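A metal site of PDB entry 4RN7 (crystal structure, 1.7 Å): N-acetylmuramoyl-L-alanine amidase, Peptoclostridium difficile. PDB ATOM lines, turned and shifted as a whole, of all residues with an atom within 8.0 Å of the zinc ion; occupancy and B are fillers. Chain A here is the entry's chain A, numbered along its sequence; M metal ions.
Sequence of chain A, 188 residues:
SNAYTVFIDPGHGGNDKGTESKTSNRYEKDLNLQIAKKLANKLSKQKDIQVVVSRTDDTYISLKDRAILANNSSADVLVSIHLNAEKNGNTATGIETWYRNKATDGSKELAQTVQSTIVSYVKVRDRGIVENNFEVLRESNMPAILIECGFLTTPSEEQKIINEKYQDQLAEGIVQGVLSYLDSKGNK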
ATOM      1  N   PRO A  10      19.464  17.375 -18.501  1.00  0.00           N
ATOM      2  CA  PRO A  10      19.208  16.025 -18.010  1.00  0.00           C
ATOM      3  C   PRO A  10      19.803  15.865 -16.613  1.00  0.00           C
ATOM      4  O   PRO A  10      21.017  15.943 -16.449  1.00  0.00           O
ATOM      5  CB  PRO A  10      19.951  15.118 -19.002  1.00  0.00           C
ATOM      6  CG  PRO A  10      20.544  16.053 -20.083  1.00  0.00           C
ATOM      7  CD  PRO A  10      20.556  17.439 -19.488  1.00  0.00           C
ATOM      8  N   GLY A  11      18.959  15.638 -15.609  1.00  0.00           N
ATOM      9  CA  GLY A  11      19.415  15.664 -14.232  1.00  0.00           C
ATOM     10  C   GLY A  11      20.478  14.616 -13.937  1.00  0.00           C
ATOM     11  O   GLY A  11      20.503  13.548 -14.552  1.00  0.00           O
ATOM     12  N   HIS A  12      21.348  14.950 -12.993  1.00  0.00           N
ATOM     13  CA  HIS A  12      22.388  14.036 -12.518  1.00  0.00           C
ATOM     14  C   HIS A  12      23.398  13.718 -13.630  1.00  0.00           C
ATOM     15  O   HIS A  12      23.441  14.419 -14.643  1.00  0.00           O
ATOM     16  CB  HIS A  12      21.738  12.785 -11.902  1.00  0.00           C
ATOM     17  CG  HIS A  12      20.653  13.119 -10.913  1.00  0.00           C
ATOM     18  ND1 HIS A  12      20.922  13.457  -9.614  1.00  0.00           N
ATOM     19  CD2 HIS A  12      19.313  13.185 -11.053  1.00  0.00           C
ATOM     20  CE1 HIS A  12      19.790  13.701  -8.980  1.00  0.00           C
ATOM     21  NE2 HIS A  12      18.797  13.559  -9.838  1.00  0.00           N
ATOM     22  N   ASP A  16      27.141  11.184  -9.992  1.00  0.00           N
ATOM     23  CA  ASP A  16      25.827  11.375  -9.400  1.00  0.00           C
ATOM     24  C   ASP A  16      24.801  10.544 -10.175  1.00  0.00           C
ATOM     25  O   ASP A  16      24.305  10.959 -11.211  1.00  0.00           O
ATOM     26  CB  ASP A  16      25.427  12.854  -9.405  1.00  0.00           C
ATOM     27  CG  ASP A  16      24.013  13.088  -8.860  1.00  0.00           C
ATOM     28  OD1 ASP A  16      23.428  12.145  -8.276  1.00  0.00           O
ATOM     29  OD2 ASP A  16      23.482  14.197  -9.008  1.00  0.00           O
ATOM     30  N   LYS A  17      24.475   9.363  -9.641  1.00  0.00           N
ATOM     31  CA  LYS A  17      23.571   8.457 -10.337  1.00  0.00           C
ATOM     32  C   LYS A  17      22.098   8.853 -10.216  1.00  0.00           C
ATOM     33  O   LYS A  17      21.261   8.384 -10.988  1.00  0.00           O
ATOM     34  CB  LYS A  17      23.737   7.024  -9.804  1.00  0.00           C
ATOM     35  CG  LYS A  17      25.149   6.445  -9.973  1.00  0.00           C
ATOM     36  CD  LYS A  17      25.286   5.098  -9.271  1.00  0.00           C
ATOM     37  N   GLY A  18      21.772   9.707  -9.256  1.00  0.00           N
ATOM     38  CA  GLY A  18      20.352   9.971  -8.990  1.00  0.00           C
ATOM     39  C   GLY A  18      19.739   8.737  -8.364  1.00  0.00           C
ATOM     40  O   GLY A  18      20.450   7.903  -7.811  1.00  0.00           O
ATOM     41  N   THR A  19      18.414   8.598  -8.453  1.00  0.00           N
ATOM     42  CA  THR A  19      17.765   7.443  -7.866  1.00  0.00           C
ATOM     43  C   THR A  19      18.179   6.157  -8.583  1.00  0.00           C
ATOM     44  O   THR A  19      18.435   6.166  -9.789  1.00  0.00           O
ATOM     45  CB  THR A  19      16.232   7.596  -7.916  1.00  0.00           C
ATOM     46  OG1 THR A  19      15.874   8.864  -7.350  1.00  0.00           O
ATOM     47  CG2 THR A  19      15.555   6.488  -7.140  1.00  0.00           C
ATOM     48  N   GLU A  28      18.671   6.681 -12.521  1.00  0.00           N
ATOM     49  CA  GLU A  28      17.992   7.881 -13.010  1.00  0.00           C
ATOM     50  C   GLU A  28      18.837   8.692 -13.993  1.00  0.00           C
ATOM     51  O   GLU A  28      18.321   9.147 -15.007  1.00  0.00           O
ATOM     52  CB  GLU A  28      17.573   8.762 -11.823  1.00  0.00           C
ATOM     53  CG  GLU A  28      17.065  10.145 -12.243  1.00  0.00           C
ATOM     54  CD  GLU A  28      16.777  11.039 -11.050  1.00  0.00           C
ATOM     55  OE1 GLU A  28      16.870  10.559  -9.890  1.00  0.00           O
ATOM     56  OE2 GLU A  28      16.441  12.226 -11.266  1.00  0.00           O
ATOM     57  N   LYS A  29      20.136   8.848 -13.713  1.00  0.00           N
ATOM     58  CA  LYS A  29      20.987   9.645 -14.589  1.00  0.00           C
ATOM     59  C   LYS A  29      20.904   9.178 -16.046  1.00  0.00           C
ATOM     60  O   LYS A  29      20.912  10.007 -16.955  1.00  0.00           O
ATOM     61  CB  LYS A  29      22.455   9.644 -14.126  1.00  0.00           C
ATOM     62  CG  LYS A  29      23.133   8.271 -14.135  1.00  0.00           C
ATOM     63  CD  LYS A  29      24.666   8.423 -14.046  1.00  0.00           C
ATOM     64  CE  LYS A  29      25.371   7.072 -14.193  1.00  0.00           C
ATOM     65  NZ  LYS A  29      26.863   7.172 -14.128  1.00  0.00           N
ATOM     66  N   ASN A  32      17.261   9.802 -17.507  1.00  0.00           N
ATOM     67  CA  ASN A  32      17.134  11.233 -17.772  1.00  0.00           C
ATOM     68  C   ASN A  32      17.771  11.622 -19.116  1.00  0.00           C
ATOM     69  O   ASN A  32      17.194  12.409 -19.868  1.00  0.00           O
ATOM     70  CB  ASN A  32      17.826  12.032 -16.667  1.00  0.00           C
ATOM     71  CG  ASN A  32      17.047  12.042 -15.362  1.00  0.00           C
ATOM     72  OD1 ASN A  32      15.882  11.614 -15.283  1.00  0.00           O
ATOM     73  ND2 ASN A  32      17.711  12.539 -14.305  1.00  0.00           N
ATOM     74  N   SER A  80      14.457  21.031 -17.091  1.00  0.00           N
ATOM     75  CA  SER A  80      15.284  20.022 -16.446  1.00  0.00           C
ATOM     76  C   SER A  80      14.485  18.730 -16.412  1.00  0.00           C
ATOM     77  O   SER A  80      13.272  18.749 -16.152  1.00  0.00           O
ATOM     78  CB  SER A  80      15.651  20.453 -15.025  1.00  0.00           C
ATOM     79  OG  SER A  80      16.563  19.539 -14.435  1.00  0.00           O
ATOM     80  N   ILE A  81      15.153  17.618 -16.685  1.00  0.00           N
ATOM     81  CA  ILE A  81      14.475  16.319 -16.769  1.00  0.00           C
ATOM     82  C   ILE A  81      14.977  15.419 -15.643  1.00  0.00           C
ATOM     83  O   ILE A  81      16.165  15.100 -15.593  1.00  0.00           O
ATOM     84  CB  ILE A  81      14.789  15.642 -18.121  1.00  0.00           C
ATOM     85  CG1 ILE A  81      14.224  16.499 -19.279  1.00  0.00           C
ATOM     86  CG2 ILE A  81      14.219  14.238 -18.164  1.00  0.00           C
ATOM     87  CD1 ILE A  81      12.691  16.624 -19.248  1.00  0.00           C
ATOM     88  N   HIS A  82      14.078  15.012 -14.753  1.00  0.00           N
ATOM     89  CA  HIS A  82      14.435  14.165 -13.619  1.00  0.00           C
ATOM     90  C   HIS A  82      13.405  13.052 -13.487  1.00  0.00           C
ATOM     91  O   HIS A  82      12.406  13.064 -14.187  1.00  0.00           O
ATOM     92  CB  HIS A  82      14.428  14.963 -12.318  1.00  0.00           C
ATOM     93  CG  HIS A  82      15.683  15.754 -12.077  1.00  0.00           C
ATOM     94  ND1 HIS A  82      16.567  15.419 -11.077  1.00  0.00           N
ATOM     95  CD2 HIS A  82      16.197  16.851 -12.695  1.00  0.00           C
ATOM     96  CE1 HIS A  82      17.568  16.284 -11.078  1.00  0.00           C
ATOM     97  NE2 HIS A  82      17.366  17.166 -12.046  1.00  0.00           N
ATOM     98  N   LEU A  83      13.653  12.082 -12.606  1.00  0.00           N
ATOM     99  CA  LEU A  83      12.639  11.089 -12.241  1.00  0.00           C
ATOM    100  C   LEU A  83      12.411  11.228 -10.749  1.00  0.00           C
ATOM    101  O   LEU A  83      13.322  11.539  -9.981  1.00  0.00           O
ATOM    102  CB  LEU A  83      13.082   9.663 -12.554  1.00  0.00           C
ATOM    103  CG  LEU A  83      13.500   9.380 -14.003  1.00  0.00           C
ATOM    104  CD1 LEU A  83      14.013   7.940 -14.143  1.00  0.00           C
ATOM    105  CD2 LEU A  83      12.331   9.625 -14.935  1.00  0.00           C
ATOM    106  N   ASN A  84      11.181  10.987 -10.316  1.00  0.00           N
ATOM    107  CA  ASN A  84      10.863  11.165  -8.930  1.00  0.00           C
ATOM    108  C   ASN A  84      11.274   9.931  -8.124  1.00  0.00           C
ATOM    109  O   ASN A  84      11.561   8.855  -8.671  1.00  0.00           O
ATOM    110  CB  ASN A  84       9.366  11.430  -8.782  1.00  0.00           C
ATOM    111  CG  ASN A  84       9.066  12.487  -7.730  1.00  0.00           C
ATOM    112  OD1 ASN A  84       9.746  12.564  -6.715  1.00  0.00           O
ATOM    113  ND2 ASN A  84       8.050  13.313  -7.981  1.00  0.00           N
ATOM    114  N   ALA A  85      11.301  10.097  -6.806  1.00  0.00           N
ATOM    115  CA  ALA A  85      11.608   8.992  -5.912  1.00  0.00           C
ATOM    116  C   ALA A  85      10.889   9.197  -4.592  1.00  0.00           C
ATOM    117  O   ALA A  85      10.824  10.315  -4.088  1.00  0.00           O
ATOM    118  CB  ALA A  85      13.110   8.903  -5.668  1.00  0.00           C
ATOM    119  N   TRP A  98       7.956  21.142 -11.523  1.00  0.00           N
ATOM    120  CA  TRP A  98       8.363  22.137 -10.548  1.00  0.00           C
ATOM    121  C   TRP A  98       8.731  23.466 -11.213  1.00  0.00           C
ATOM    122  O   TRP A  98       9.178  23.484 -12.364  1.00  0.00           O
ATOM    123  CB  TRP A  98       9.617  21.670  -9.801  1.00  0.00           C
ATOM    124  CG  TRP A  98       9.478  20.396  -9.030  1.00  0.00           C
ATOM    125  CD1 TRP A  98       8.360  19.639  -8.843  1.00  0.00           C
ATOM    126  CD2 TRP A  98      10.537  19.729  -8.322  1.00  0.00           C
ATOM    127  NE1 TRP A  98       8.654  18.542  -8.058  1.00  0.00           N
ATOM    128  CE2 TRP A  98       9.988  18.577  -7.736  1.00  0.00           C
ATOM    129  CE3 TRP A  98      11.894  20.005  -8.133  1.00  0.00           C
ATOM    130  CZ2 TRP A  98      10.759  17.693  -6.960  1.00  0.00           C
ATOM    131  CZ3 TRP A  98      12.654  19.120  -7.365  1.00  0.00           C
ATOM    132  CH2 TRP A  98      12.086  17.991  -6.791  1.00  0.00           C
ATOM    133  N   PHE A 134      14.824  24.188  -5.799  1.00  0.00           N
ATOM    134  CA  PHE A 134      15.947  23.517  -6.464  1.00  0.00           C
ATOM    135  C   PHE A 134      16.890  24.525  -7.127  1.00  0.00           C
ATOM    136  O   PHE A 134      16.443  25.388  -7.889  1.00  0.00           O
ATOM    137  CB  PHE A 134      15.405  22.530  -7.497  1.00  0.00           C
ATOM    138  CG  PHE A 134      16.457  21.657  -8.129  1.00  0.00           C
ATOM    139  CD1 PHE A 134      17.190  20.755  -7.361  1.00  0.00           C
ATOM    140  CD2 PHE A 134      16.676  21.704  -9.507  1.00  0.00           C
ATOM    141  CE1 PHE A 134      18.147  19.934  -7.957  1.00  0.00           C
ATOM    142  CE2 PHE A 134      17.626  20.875 -10.104  1.00  0.00           C
ATOM    143  CZ  PHE A 134      18.363  19.997  -9.331  1.00  0.00           C
ATOM    144  N   LEU A 146      11.278  21.965 -13.898  1.00  0.00           N
ATOM    145  CA  LEU A 146      11.912  20.666 -13.743  1.00  0.00           C
ATOM    146  C   LEU A 146      10.773  19.670 -13.766  1.00  0.00           C
ATOM    147  O   LEU A 146       9.840  19.779 -12.976  1.00  0.00           O
ATOM    148  CB  LEU A 146      12.688  20.569 -12.418  1.00  0.00           C
ATOM    149  CG  LEU A 146      13.395  19.229 -12.102  1.00  0.00           C
ATOM    150  CD1 LEU A 146      14.628  19.477 -11.234  1.00  0.00           C
ATOM    151  CD2 LEU A 146      12.461  18.218 -11.416  1.00  0.00           C
ATOM    152  N   ILE A 147      10.835  18.722 -14.707  1.00  0.00           N
ATOM    153  CA  ILE A 147       9.781  17.729 -14.814  1.00  0.00           C
ATOM    154  C   ILE A 147      10.231  16.447 -14.145  1.00  0.00           C
ATOM    155  O   ILE A 147      11.259  15.886 -14.527  1.00  0.00           O
ATOM    156  CB  ILE A 147       9.439  17.431 -16.274  1.00  0.00           C
ATOM    157  CG1 ILE A 147       9.231  18.731 -17.054  1.00  0.00           C
ATOM    158  CG2 ILE A 147       8.144  16.593 -16.347  1.00  0.00           C
ATOM    159  CD1 ILE A 147       9.172  18.550 -18.569  1.00  0.00           C
ATOM    160  N   GLU A 148       9.437  15.967 -13.177  1.00  0.00           N
ATOM    161  CA  GLU A 148       9.688  14.692 -12.510  1.00  0.00           C
ATOM    162  C   GLU A 148       8.882  13.638 -13.264  1.00  0.00           C
ATOM    163  O   GLU A 148       7.675  13.515 -13.071  1.00  0.00           O
ATOM    164  CB  GLU A 148       9.263  14.729 -11.037  1.00  0.00           C
ATOM    165  CG  GLU A 148      10.094  15.684 -10.150  1.00  0.00           C
ATOM    166  CD  GLU A 148      11.472  15.137  -9.813  1.00  0.00           C
ATOM    167  OE1 GLU A 148      11.886  14.127 -10.410  1.00  0.00           O
ATOM    168  OE2 GLU A 148      12.161  15.720  -8.953  1.00  0.00           O
HETATM  169 ZN    ZN M   1      16.680  13.771  -9.817  1.00  0.00          ZN
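ND1 of His 12 sits at hydrogen-bond distance from OD2 of Asp 16 (2.7 Å).
N of His 82 is in hydrogen-bond range of O of Ile 147, 3.0 Å away.
NE2 of His 82 sits close to OG of Ser 80, 3.5 Å away.
The backbone NH of Glu 28 lies within hydrogen-bond range of the backbone carbonyl oxygen of Thr 19 (2.8 Å).
The backbone carbonyl oxygen (O) of Glu 28 lies close to the side-chain amide oxygen (OD1) of Asn 32 (3.5 Å).
O of Lys 17 sits at hydrogen-bond distance from N of Glu 28 (3.5 Å).
OE2 of Glu 28 sits close to N of Leu 83 (3.1 Å).
Three residues have an atom within 4 Å of the zinc ion: His 12, Glu 28 and His 82.
The zinc ion is bound by a ring nitrogen (ND1) of His 82 (2.1 Å), a ring nitrogen (NE2) of His 12 (2.1 Å) and the side-chain carboxylate of Glu 28 (2.1 Å).
The zinc ion has three donor atoms within binding distance.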
